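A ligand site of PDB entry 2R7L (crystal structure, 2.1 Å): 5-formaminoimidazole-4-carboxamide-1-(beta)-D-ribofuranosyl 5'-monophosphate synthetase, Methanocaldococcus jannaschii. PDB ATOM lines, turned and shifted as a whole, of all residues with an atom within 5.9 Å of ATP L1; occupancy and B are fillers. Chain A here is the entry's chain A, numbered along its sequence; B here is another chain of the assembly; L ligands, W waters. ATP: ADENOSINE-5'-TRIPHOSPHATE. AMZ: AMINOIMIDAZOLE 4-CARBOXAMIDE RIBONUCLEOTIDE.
Water W5 lies within hydrogen-bond range of O1A of ATP L1 (2.5 Å), OE1 of Glu 310 (2.7 Å) and NH2 of Arg 125 (3.3 Å).
Water W2 lies within hydrogen-bond range of O3G of ATP L1 (2.6 Å), OE2 of Glu 230 (2.6 Å) and O of Tyr 253 (3.0 Å).
Water W7 lies within hydrogen-bond range of O2G of ATP L1 (2.7 Å), NE2 of Gln 297 (2.9 Å) and NE of Arg 228 (3.1 Å).
Water W3 lies within hydrogen-bond range of an oxygen (O2') of ATP L1 (2.8 Å) and the guanidinium group (NH1) of Arg 238 of chain B (3.3 Å).
Water W1 lies within hydrogen-bond range of OH of Tyr 201 (2.8 Å), N3 of ATP L1 (3.1 Å) and NH1 of Arg 238 of chain B (3.2 Å).
Water W6 lies within hydrogen-bond range of N of Ile 255 (3.2 Å) and O3G of ATP L1 (3.3 Å).
NZ of Lys 156 lies within salt-bridge range of OE2 of Glu 199 (2.8 Å).
OE1 of Gln 297 sits at hydrogen-bond distance from N of Met 311, 3.4 Å away.
The backbone carbonyl oxygen (O) of Glu 310 lies within hydrogen-bond range of the backbone NH (N) of Gln 297 (3.0 Å).
NE2 of Gln 297 sits close to NH2 of Arg 228 (3.2 Å).
The backbone carbonyl oxygen (O) of Glu 199 is in hydrogen-bond range of the backbone NH (N) of Ile 154, 2.8 Å away.
The backbone carbonyl oxygen (O) of Gln 297 sits at hydrogen-bond distance from the backbone NH (N) of Phe 309, at 3.0 Å.
OE1 of Glu 230 lies within salt-bridge range of NH2 of Arg 238 of chain B, 2.7 Å away.
N of Arg 228 lies within hydrogen-bond range of OD1 of Asn 206 (2.9 Å).
An oxygen (O3') of ATP L1 is in hydrogen-bond range of the side-chain carboxylate (OE2) of Glu 230 (2.4 Å).
NE2 of Gln 297 is in hydrogen-bond range of O1B of ATP L1.
N6 of ATP L1 is in hydrogen-bond range of OE2 of Glu 199 (2.8 Å).
The guanidinium group of Arg 238 of chain B is in hydrogen-bond range of an oxygen (O2') of ATP L1 (2.9 Å).
N6 of ATP L1 is in hydrogen-bond range of O of Glu 200.
NZ of Lys 156 lies within salt-bridge range of O1A of ATP L1 (2.9 Å).
NH2 of Arg 228 is in salt-bridge range of O2G of ATP L1 (3.4 Å).
N of Val 202 lies within hydrogen-bond range of N1 of ATP L1 (2.9 Å).
The side-chain hydroxyl (OH) of Tyr 166 lies within hydrogen-bond range of an oxygen (O2A) of ATP L1, at 2.5 Å.
Residues that only touch ATP L1: Pro 140 (3.6 Å), Ile 154 (3.7 Å), Tyr 201 (3.6 Å), Tyr 253 (3.7 Å), Ile 255 (3.4 Å), Leu 299 (3.6 Å), Phe 309 (3.7 Å) and Glu 310 (3.5 Å).
Hydrophobic or aromatic side chains that line ATP L1: Pro 140, Ile 154, Tyr 166, Tyr 201, Val 202, Tyr 253, Ile 255, Leu 299 and Phe 309.
Of the 23 residues printed, 17 come within 4 Å of ATP L1.
An oxygen (O1) of AMZ L2 is in hydrogen-bond range of an oxygen (O1G) of ATP L1, at 2.4 Å.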
ATOM      1  N   ARG A 125     -23.384 -17.053   3.620  1.00  0.00           N
ATOM      2  CA  ARG A 125     -22.788 -18.381   3.656  1.00  0.00           C
ATOM      3  C   ARG A 125     -23.761 -19.475   4.121  1.00  0.00           C
ATOM      4  O   ARG A 125     -23.708 -20.611   3.637  1.00  0.00           O
ATOM      5  CB  ARG A 125     -21.550 -18.351   4.557  1.00  0.00           C
ATOM      6  CG  ARG A 125     -20.678 -19.596   4.489  1.00  0.00           C
ATOM      7  CD  ARG A 125     -19.442 -19.462   5.383  1.00  0.00           C
ATOM      8  NE  ARG A 125     -18.489 -18.463   4.892  1.00  0.00           N
ATOM      9  CZ  ARG A 125     -17.617 -18.660   3.907  1.00  0.00           C
ATOM     10  NH1 ARG A 125     -17.573 -19.824   3.273  1.00  0.00           N
ATOM     11  NH2 ARG A 125     -16.787 -17.685   3.545  1.00  0.00           N
ATOM     12  N   PRO A 140     -17.198 -29.031   0.956  1.00  0.00           N
ATOM     13  CA  PRO A 140     -16.146 -29.283   1.943  1.00  0.00           C
ATOM     14  C   PRO A 140     -16.740 -29.413   3.356  1.00  0.00           C
ATOM     15  O   PRO A 140     -17.696 -28.707   3.682  1.00  0.00           O
ATOM     16  CB  PRO A 140     -15.279 -28.022   1.870  1.00  0.00           C
ATOM     17  CG  PRO A 140     -15.638 -27.364   0.557  1.00  0.00           C
ATOM     18  CD  PRO A 140     -17.076 -27.692   0.345  1.00  0.00           C
ATOM     19  N   ILE A 154      -8.677 -24.951   5.215  1.00  0.00           N
ATOM     20  CA  ILE A 154      -8.470 -23.571   4.793  1.00  0.00           C
ATOM     21  C   ILE A 154      -9.350 -22.694   5.672  1.00  0.00           C
ATOM     22  O   ILE A 154     -10.465 -23.072   6.032  1.00  0.00           O
ATOM     23  CB  ILE A 154      -8.777 -23.363   3.284  1.00  0.00           C
ATOM     24  CG1 ILE A 154      -8.459 -21.924   2.852  1.00  0.00           C
ATOM     25  CG2 ILE A 154     -10.209 -23.728   2.970  1.00  0.00           C
ATOM     26  CD1 ILE A 154      -8.378 -21.737   1.333  1.00  0.00           C
ATOM     27  N   LYS A 156     -11.146 -18.985   6.176  1.00  0.00           N
ATOM     28  CA  LYS A 156     -11.610 -17.805   5.463  1.00  0.00           C
ATOM     29  C   LYS A 156     -12.211 -16.758   6.409  1.00  0.00           C
ATOM     30  O   LYS A 156     -12.714 -17.093   7.480  1.00  0.00           O
ATOM     31  CB  LYS A 156     -12.656 -18.209   4.415  1.00  0.00           C
ATOM     32  CG  LYS A 156     -12.156 -19.255   3.427  1.00  0.00           C
ATOM     33  CD  LYS A 156     -13.281 -19.765   2.554  1.00  0.00           C
ATOM     34  CE  LYS A 156     -12.743 -20.655   1.445  1.00  0.00           C
ATOM     35  NZ  LYS A 156     -13.830 -21.369   0.689  1.00  0.00           N
ATOM     36  N   TYR A 166      -6.602 -15.235   4.135  1.00  0.00           N
ATOM     37  CA  TYR A 166      -6.742 -16.684   4.243  1.00  0.00           C
ATOM     38  C   TYR A 166      -5.468 -17.361   4.752  1.00  0.00           C
ATOM     39  O   TYR A 166      -4.368 -16.805   4.649  1.00  0.00           O
ATOM     40  CB  TYR A 166      -7.096 -17.277   2.870  1.00  0.00           C
ATOM     41  CG  TYR A 166      -8.481 -16.930   2.359  1.00  0.00           C
ATOM     42  CD1 TYR A 166      -9.130 -15.760   2.750  1.00  0.00           C
ATOM     43  CD2 TYR A 166      -9.148 -17.765   1.469  1.00  0.00           C
ATOM     44  CE1 TYR A 166     -10.394 -15.435   2.288  1.00  0.00           C
ATOM     45  CE2 TYR A 166     -10.412 -17.461   1.000  1.00  0.00           C
ATOM     46  CZ  TYR A 166     -11.037 -16.292   1.412  1.00  0.00           C
ATOM     47  OH  TYR A 166     -12.292 -15.977   0.953  1.00  0.00           O
ATOM     48  N   GLU A 199     -12.876 -24.752   6.922  1.00  0.00           N
ATOM     49  CA  GLU A 199     -13.384 -25.899   6.173  1.00  0.00           C
ATOM     50  C   GLU A 199     -12.285 -26.776   5.616  1.00  0.00           C
ATOM     51  O   GLU A 199     -11.137 -26.351   5.457  1.00  0.00           O
ATOM     52  CB  GLU A 199     -14.328 -25.456   5.039  1.00  0.00           C
ATOM     53  CG  GLU A 199     -13.690 -24.515   4.016  1.00  0.00           C
ATOM     54  CD  GLU A 199     -14.606 -24.213   2.825  1.00  0.00           C
ATOM     55  OE1 GLU A 199     -15.845 -24.233   2.996  1.00  0.00           O
ATOM     56  OE2 GLU A 199     -14.079 -23.963   1.726  1.00  0.00           O
ATOM     57  N   GLU A 200     -12.649 -28.010   5.316  1.00  0.00           N
ATOM     58  CA  GLU A 200     -11.749 -28.961   4.701  1.00  0.00           C
ATOM     59  C   GLU A 200     -11.030 -28.362   3.492  1.00  0.00           C
ATOM     60  O   GLU A 200     -11.650 -27.813   2.589  1.00  0.00           O
ATOM     61  CB  GLU A 200     -12.557 -30.175   4.263  1.00  0.00           C
ATOM     62  CG  GLU A 200     -11.796 -31.163   3.410  1.00  0.00           C
ATOM     63  CD  GLU A 200     -12.667 -32.272   2.894  1.00  0.00           C
ATOM     64  OE1 GLU A 200     -13.917 -32.152   3.012  1.00  0.00           O
ATOM     65  OE2 GLU A 200     -12.119 -33.273   2.395  1.00  0.00           O
ATOM     66  N   TYR A 201      -9.701 -28.441   3.493  1.00  0.00           N
ATOM     67  CA  TYR A 201      -8.941 -28.075   2.304  1.00  0.00           C
ATOM     68  C   TYR A 201      -9.129 -29.216   1.301  1.00  0.00           C
ATOM     69  O   TYR A 201      -8.691 -30.332   1.552  1.00  0.00           O
ATOM     70  CB  TYR A 201      -7.464 -27.879   2.640  1.00  0.00           C
ATOM     71  CG  TYR A 201      -6.694 -27.227   1.510  1.00  0.00           C
ATOM     72  CD1 TYR A 201      -6.421 -25.870   1.534  1.00  0.00           C
ATOM     73  CD2 TYR A 201      -6.270 -27.963   0.410  1.00  0.00           C
ATOM     74  CE1 TYR A 201      -5.726 -25.258   0.493  1.00  0.00           C
ATOM     75  CE2 TYR A 201      -5.579 -27.365  -0.632  1.00  0.00           C
ATOM     76  CZ  TYR A 201      -5.306 -26.010  -0.584  1.00  0.00           C
ATOM     77  OH  TYR A 201      -4.629 -25.402  -1.612  1.00  0.00           O
ATOM     78  N   VAL A 202      -9.805 -28.934   0.188  1.00  0.00           N
ATOM     79  CA  VAL A 202      -9.996 -29.948  -0.840  1.00  0.00           C
ATOM     80  C   VAL A 202      -8.824 -29.910  -1.805  1.00  0.00           C
ATOM     81  O   VAL A 202      -8.481 -28.850  -2.320  1.00  0.00           O
ATOM     82  CB  VAL A 202     -11.323 -29.776  -1.600  1.00  0.00           C
ATOM     83  CG1 VAL A 202     -11.410 -30.776  -2.758  1.00  0.00           C
ATOM     84  CG2 VAL A 202     -12.527 -29.958  -0.653  1.00  0.00           C
ATOM     85  N   VAL A 203      -8.207 -31.049  -2.042  1.00  0.00           N
ATOM     86  CA  VAL A 203      -7.029 -31.089  -2.895  1.00  0.00           C
ATOM     87  C   VAL A 203      -7.389 -31.613  -4.283  1.00  0.00           C
ATOM     88  O   VAL A 203      -7.541 -32.817  -4.484  1.00  0.00           O
ATOM     89  CB  VAL A 203      -5.882 -31.913  -2.266  1.00  0.00           C
ATOM     90  CG1 VAL A 203      -4.607 -31.767  -3.097  1.00  0.00           C
ATOM     91  CG2 VAL A 203      -5.638 -31.472  -0.834  1.00  0.00           C
ATOM     92  N   ASN A 206      -9.304 -27.136 -10.081  1.00  0.00           N
ATOM     93  CA  ASN A 206     -10.369 -26.141 -10.111  1.00  0.00           C
ATOM     94  C   ASN A 206     -11.144 -26.090 -11.442  1.00  0.00           C
ATOM     95  O   ASN A 206     -10.555 -25.925 -12.520  1.00  0.00           O
ATOM     96  CB  ASN A 206      -9.794 -24.763  -9.816  1.00  0.00           C
ATOM     97  CG  ASN A 206     -10.858 -23.682  -9.737  1.00  0.00           C
ATOM     98  OD1 ASN A 206     -10.611 -22.537 -10.114  1.00  0.00           O
ATOM     99  ND2 ASN A 206     -12.053 -24.030  -9.239  1.00  0.00           N
ATOM    100  N   ARG A 228      -9.323 -20.455 -11.752  1.00  0.00           N
ATOM    101  CA  ARG A 228      -8.916 -19.157 -11.229  1.00  0.00           C
ATOM    102  C   ARG A 228      -7.421 -18.961 -11.340  1.00  0.00           C
ATOM    103  O   ARG A 228      -6.658 -19.923 -11.292  1.00  0.00           O
ATOM    104  CB  ARG A 228      -9.324 -19.018  -9.757  1.00  0.00           C
ATOM    105  CG  ARG A 228     -10.789 -19.223  -9.482  1.00  0.00           C
ATOM    106  CD  ARG A 228     -11.631 -18.251 -10.279  1.00  0.00           C
ATOM    107  NE  ARG A 228     -12.853 -17.892  -9.570  1.00  0.00           N
ATOM    108  CZ  ARG A 228     -14.004 -17.606 -10.170  1.00  0.00           C
ATOM    109  NH1 ARG A 228     -14.099 -17.626 -11.489  1.00  0.00           N
ATOM    110  NH2 ARG A 228     -15.074 -17.289  -9.439  1.00  0.00           N
ATOM    111  N   GLU A 230      -4.962 -16.707  -9.249  1.00  0.00           N
ATOM    112  CA  GLU A 230      -5.003 -15.930  -8.015  1.00  0.00           C
ATOM    113  C   GLU A 230      -3.613 -15.506  -7.520  1.00  0.00           C
ATOM    114  O   GLU A 230      -2.642 -16.230  -7.699  1.00  0.00           O
ATOM    115  CB  GLU A 230      -5.766 -16.732  -6.943  1.00  0.00           C
ATOM    116  CG  GLU A 230      -7.251 -16.869  -7.257  1.00  0.00           C
ATOM    117  CD  GLU A 230      -7.937 -17.998  -6.526  1.00  0.00           C
ATOM    118  OE1 GLU A 230      -7.243 -18.948  -6.093  1.00  0.00           O
ATOM    119  OE2 GLU A 230      -9.182 -17.952  -6.407  1.00  0.00           O
ATOM    120  N   TYR A 253      -5.177 -15.174  -1.790  1.00  0.00           N
ATOM    121  CA  TYR A 253      -5.995 -15.756  -2.843  1.00  0.00           C
ATOM    122  C   TYR A 253      -6.849 -14.694  -3.546  1.00  0.00           C
ATOM    123  O   TYR A 253      -8.033 -14.876  -3.755  1.00  0.00           O
ATOM    124  CB  TYR A 253      -6.861 -16.881  -2.261  1.00  0.00           C
ATOM    125  CG  TYR A 253      -6.043 -18.023  -1.705  1.00  0.00           C
ATOM    126  CD1 TYR A 253      -5.911 -19.210  -2.419  1.00  0.00           C
ATOM    127  CD2 TYR A 253      -5.388 -17.913  -0.484  1.00  0.00           C
ATOM    128  CE1 TYR A 253      -5.153 -20.263  -1.933  1.00  0.00           C
ATOM    129  CE2 TYR A 253      -4.624 -18.963   0.023  1.00  0.00           C
ATOM    130  CZ  TYR A 253      -4.512 -20.135  -0.710  1.00  0.00           C
ATOM    131  OH  TYR A 253      -3.764 -21.178  -0.227  1.00  0.00           O
ATOM    132  N   VAL A 254      -6.211 -13.588  -3.903  1.00  0.00           N
ATOM    133  CA  VAL A 254      -6.892 -12.486  -4.576  1.00  0.00           C
ATOM    134  C   VAL A 254      -7.101 -12.813  -6.063  1.00  0.00           C
ATOM    135  O   VAL A 254      -6.127 -13.023  -6.798  1.00  0.00           O
ATOM    136  CB  VAL A 254      -6.059 -11.202  -4.484  1.00  0.00           C
ATOM    137  CG1 VAL A 254      -6.791 -10.044  -5.144  1.00  0.00           C
ATOM    138  CG2 VAL A 254      -5.739 -10.879  -3.025  1.00  0.00           C
ATOM    139  N   ILE A 255      -8.355 -12.838  -6.504  1.00  0.00           N
ATOM    140  CA  ILE A 255      -8.644 -13.136  -7.915  1.00  0.00           C
ATOM    141  C   ILE A 255      -8.015 -12.100  -8.832  1.00  0.00           C
ATOM    142  O   ILE A 255      -8.256 -10.890  -8.683  1.00  0.00           O
ATOM    143  CB  ILE A 255     -10.170 -13.248  -8.219  1.00  0.00           C
ATOM    144  CG1 ILE A 255     -10.381 -13.863  -9.610  1.00  0.00           C
ATOM    145  CG2 ILE A 255     -10.869 -11.889  -8.140  1.00  0.00           C
ATOM    146  CD1 ILE A 255      -9.828 -15.274  -9.741  1.00  0.00           C
ATOM    147  N   GLN A 297     -18.443 -23.178  -8.339  1.00  0.00           N
ATOM    148  CA  GLN A 297     -16.996 -23.130  -8.222  1.00  0.00           C
ATOM    149  C   GLN A 297     -16.526 -24.360  -7.464  1.00  0.00           C
ATOM    150  O   GLN A 297     -16.753 -24.492  -6.277  1.00  0.00           O
ATOM    151  CB  GLN A 297     -16.559 -21.867  -7.492  1.00  0.00           C
ATOM    152  CG  GLN A 297     -16.976 -20.596  -8.212  1.00  0.00           C
ATOM    153  CD  GLN A 297     -17.102 -19.423  -7.283  1.00  0.00           C
ATOM    154  OE1 GLN A 297     -18.209 -18.991  -6.980  1.00  0.00           O
ATOM    155  NE2 GLN A 297     -15.969 -18.907  -6.811  1.00  0.00           N
ATOM    156  N   LEU A 299     -13.879 -28.129  -6.977  1.00  0.00           N
ATOM    157  CA  LEU A 299     -12.583 -28.760  -7.030  1.00  0.00           C
ATOM    158  C   LEU A 299     -12.795 -30.238  -7.265  1.00  0.00           C
ATOM    159  O   LEU A 299     -13.618 -30.862  -6.600  1.00  0.00           O
ATOM    160  CB  LEU A 299     -11.792 -28.523  -5.742  1.00  0.00           C
ATOM    161  CG  LEU A 299     -11.305 -27.086  -5.533  1.00  0.00           C
ATOM    162  CD1 LEU A 299     -10.994 -26.798  -4.065  1.00  0.00           C
ATOM    163  CD2 LEU A 299     -10.105 -26.790  -6.421  1.00  0.00           C
ATOM    164  N   PHE A 309     -17.101 -25.378  -3.438  1.00  0.00           N
ATOM    165  CA  PHE A 309     -16.720 -24.579  -2.300  1.00  0.00           C
ATOM    166  C   PHE A 309     -17.338 -23.197  -2.381  1.00  0.00           C
ATOM    167  O   PHE A 309     -17.300 -22.424  -1.413  1.00  0.00           O
ATOM    168  CB  PHE A 309     -15.199 -24.474  -2.218  1.00  0.00           C
ATOM    169  CG  PHE A 309     -14.564 -23.788  -3.408  1.00  0.00           C
ATOM    170  CD1 PHE A 309     -14.473 -22.413  -3.454  1.00  0.00           C
ATOM    171  CD2 PHE A 309     -14.031 -24.544  -4.451  1.00  0.00           C
ATOM    172  CE1 PHE A 309     -13.872 -21.773  -4.534  1.00  0.00           C
ATOM    173  CE2 PHE A 309     -13.432 -23.909  -5.544  1.00  0.00           C
ATOM    174  CZ  PHE A 309     -13.356 -22.524  -5.577  1.00  0.00           C
ATOM    175  N   GLU A 310     -17.902 -22.874  -3.534  1.00  0.00           N
ATOM    176  CA  GLU A 310     -18.580 -21.605  -3.729  1.00  0.00           C
ATOM    177  C   GLU A 310     -19.572 -21.661  -4.891  1.00  0.00           C
ATOM    178  O   GLU A 310     -19.590 -22.619  -5.663  1.00  0.00           O
ATOM    179  CB  GLU A 310     -17.575 -20.470  -3.943  1.00  0.00           C
ATOM    180  CG  GLU A 310     -17.242 -19.676  -2.687  1.00  0.00           C
ATOM    181  CD  GLU A 310     -18.448 -18.958  -2.101  1.00  0.00           C
ATOM    182  OE1 GLU A 310     -18.373 -18.529  -0.930  1.00  0.00           O
ATOM    183  OE2 GLU A 310     -19.467 -18.800  -2.802  1.00  0.00           O
ATOM    184  N   MET A 311     -20.408 -20.631  -4.982  1.00  0.00           N
ATOM    185  CA  MET A 311     -21.365 -20.512  -6.071  1.00  0.00           C
ATOM    186  C   MET A 311     -21.818 -19.069  -6.248  1.00  0.00           C
ATOM    187  O   MET A 311     -21.656 -18.249  -5.339  1.00  0.00           O
ATOM    188  CB  MET A 311     -22.584 -21.396  -5.815  1.00  0.00           C
ATOM    189  CG  MET A 311     -23.462 -20.887  -4.703  1.00  0.00           C
ATOM    190  SD  MET A 311     -25.166 -21.459  -4.850  1.00  0.00           S
ATOM    191  CE  MET A 311     -25.828 -20.212  -5.957  1.00  0.00           C
ATOM    192  N   ASP A 316     -20.812 -15.048 -13.137  1.00  0.00           N
ATOM    193  CA  ASP A 316     -19.504 -15.102 -12.481  1.00  0.00           C
ATOM    194  C   ASP A 316     -18.403 -14.502 -13.367  1.00  0.00           C
ATOM    195  O   ASP A 316     -18.442 -14.627 -14.592  1.00  0.00           O
ATOM    196  CB  ASP A 316     -19.160 -16.542 -12.104  1.00  0.00           C
ATOM    197  CG  ASP A 316     -17.767 -16.680 -11.492  1.00  0.00           C
ATOM    198  OD1 ASP A 316     -17.676 -16.697 -10.243  1.00  0.00           O
ATOM    199  OD2 ASP A 316     -16.774 -16.748 -12.239  1.00  0.00           O
ATOM    200  N   ARG B 238      -0.211 -26.913  -5.617  1.00  0.00           N
ATOM    201  CA  ARG B 238      -0.725 -25.562  -5.417  1.00  0.00           C
ATOM    202  C   ARG B 238      -0.834 -25.239  -3.925  1.00  0.00           C
ATOM    203  O   ARG B 238      -1.302 -24.153  -3.544  1.00  0.00           O
ATOM    204  CB  ARG B 238      -2.082 -25.375  -6.102  1.00  0.00           C
ATOM    205  CG  ARG B 238      -2.449 -23.897  -6.267  1.00  0.00           C
ATOM    206  CD  ARG B 238      -3.824 -23.736  -6.860  1.00  0.00           C
ATOM    207  NE  ARG B 238      -4.071 -22.336  -7.239  1.00  0.00           N
ATOM    208  CZ  ARG B 238      -4.939 -21.539  -6.638  1.00  0.00           C
ATOM    209  NH1 ARG B 238      -5.673 -21.976  -5.624  1.00  0.00           N
ATOM    210  NH2 ARG B 238      -5.097 -20.297  -7.060  1.00  0.00           N
HETATM  211  PG  ATP L   1     -13.673 -15.124  -5.768  1.00  0.00           P
HETATM  212  O1G ATP L   1     -14.894 -14.279  -6.093  1.00  0.00           O
HETATM  213  O2G ATP L   1     -13.640 -16.461  -6.480  1.00  0.00           O
HETATM  214  O3G ATP L   1     -12.374 -14.359  -5.825  1.00  0.00           O
HETATM  215  PB  ATP L   1     -14.950 -16.535  -3.642  1.00  0.00           P
HETATM  216  O1B ATP L   1     -15.894 -16.908  -4.763  1.00  0.00           O
HETATM  217  O2B ATP L   1     -15.527 -15.981  -2.363  1.00  0.00           O
HETATM  218  O3B ATP L   1     -13.857 -15.479  -4.199  1.00  0.00           O
HETATM  219  PA  ATP L   1     -13.332 -18.173  -1.918  1.00  0.00           P
HETATM  220  O1A ATP L   1     -14.178 -19.141  -1.120  1.00  0.00           O
HETATM  221  O2A ATP L   1     -12.827 -16.893  -1.329  1.00  0.00           O
HETATM  222  O3A ATP L   1     -14.107 -17.867  -3.316  1.00  0.00           O
HETATM  223  O5' ATP L   1     -12.068 -19.015  -2.441  1.00  0.00           O
HETATM  224  C5' ATP L   1     -10.923 -18.313  -2.895  1.00  0.00           C
HETATM  225  C4' ATP L   1      -9.906 -19.348  -3.340  1.00  0.00           C
HETATM  226  O4' ATP L   1      -9.447 -20.116  -2.224  1.00  0.00           O
HETATM  227  C3' ATP L   1     -10.485 -20.366  -4.315  1.00  0.00           C
HETATM  228  O3' ATP L   1     -10.413 -19.907  -5.667  1.00  0.00           O
HETATM  229  C2' ATP L   1      -9.620 -21.587  -4.073  1.00  0.00           C
HETATM  230  O2' ATP L   1      -8.429 -21.512  -4.854  1.00  0.00           O
HETATM  231  C1' ATP L   1      -9.237 -21.480  -2.604  1.00  0.00           C
HETATM  232  N9  ATP L   1     -10.180 -22.317  -1.829  1.00  0.00           N
HETATM  233  C8  ATP L   1     -11.379 -21.903  -1.381  1.00  0.00           C
HETATM  234  N7  ATP L   1     -12.020 -22.905  -0.720  1.00  0.00           N
HETATM  235  C5  ATP L   1     -11.211 -23.983  -0.736  1.00  0.00           C
HETATM  236  C6  ATP L   1     -11.278 -25.358  -0.210  1.00  0.00           C
HETATM  237  N6  ATP L   1     -12.357 -25.798   0.469  1.00  0.00           N
HETATM  238  N1  ATP L   1     -10.222 -26.164  -0.457  1.00  0.00           N
HETATM  239  C2  ATP L   1      -9.141 -25.738  -1.154  1.00  0.00           C
HETATM  240  N3  ATP L   1      -9.012 -24.493  -1.646  1.00  0.00           N
HETATM  241  C4  ATP L   1     -10.008 -23.591  -1.488  1.00  0.00           C
HETATM  242  O5  AMZ L   2     -12.322 -12.848 -12.947  1.00  0.00           O
HETATM  243  C6  AMZ L   2     -12.947 -13.280 -11.980  1.00  0.00           C
HETATM  244  N2  AMZ L   2     -13.093 -14.576 -11.689  1.00  0.00           N
HETATM  245  C3A AMZ L   2     -13.621 -12.328 -10.998  1.00  0.00           C
HETATM  246  C7A AMZ L   2     -14.251 -12.654  -9.813  1.00  0.00           C
HETATM  247  N3  AMZ L   2     -14.409 -13.874  -9.281  1.00  0.00           N
HETATM  248  N1  AMZ L   2     -13.665 -11.010 -11.141  1.00  0.00           N
HETATM  249  C5  AMZ L   2     -14.317 -10.527 -10.079  1.00  0.00           C
HETATM  250  N   AMZ L   2     -14.671 -11.530  -9.268  1.00  0.00           N
HETATM  251  C1  AMZ L   2     -15.415 -11.409  -7.993  1.00  0.00           C
HETATM  252  C2  AMZ L   2     -14.501 -11.175  -6.790  1.00  0.00           C
HETATM  253  C3  AMZ L   2     -14.618  -9.677  -6.536  1.00  0.00           C
HETATM  254  O2  AMZ L   2     -14.564  -9.433  -5.140  1.00  0.00           O
HETATM  255  O1  AMZ L   2     -15.051 -11.897  -5.681  1.00  0.00           O
HETATM  256  O   AMZ L   2     -16.218 -10.227  -8.164  1.00  0.00           O
HETATM  257  C   AMZ L   2     -16.023  -9.363  -7.030  1.00  0.00           C
HETATM  258  C4  AMZ L   2     -16.146  -7.916  -7.556  1.00  0.00           C
HETATM  259  O3  AMZ L   2     -15.188  -7.691  -8.583  1.00  0.00           O
HETATM  260  P   AMZ L   2     -14.377  -6.330  -8.616  1.00  0.00           P
HETATM  261  OP1 AMZ L   2     -15.196  -5.115  -8.853  1.00  0.00           O
HETATM  262  O4  AMZ L   2     -13.615  -6.208  -7.203  1.00  0.00           O
HETATM  263  OP2 AMZ L   2     -13.222  -6.486  -9.733  1.00  0.00           O
HETATM  264  O   HOH W   1      -6.387 -23.940  -3.177  1.00  0.00           O
HETATM  265  O   HOH W   2     -10.315 -15.818  -5.384  1.00  0.00           O
HETATM  266  O   HOH W   3      -8.337 -23.009  -7.240  1.00  0.00           O
HETATM  267  O   HOH W   4     -18.595 -16.864  -5.388  1.00  0.00           O
HETATM  268  O   HOH W   5     -16.033 -18.396   0.389  1.00  0.00           O
HETATM  269  O   HOH W   6     -10.716 -11.840  -4.542  1.00  0.00           O
HETATM  270  O   HOH W   7     -13.109 -19.110  -6.736  1.00  0.00           O
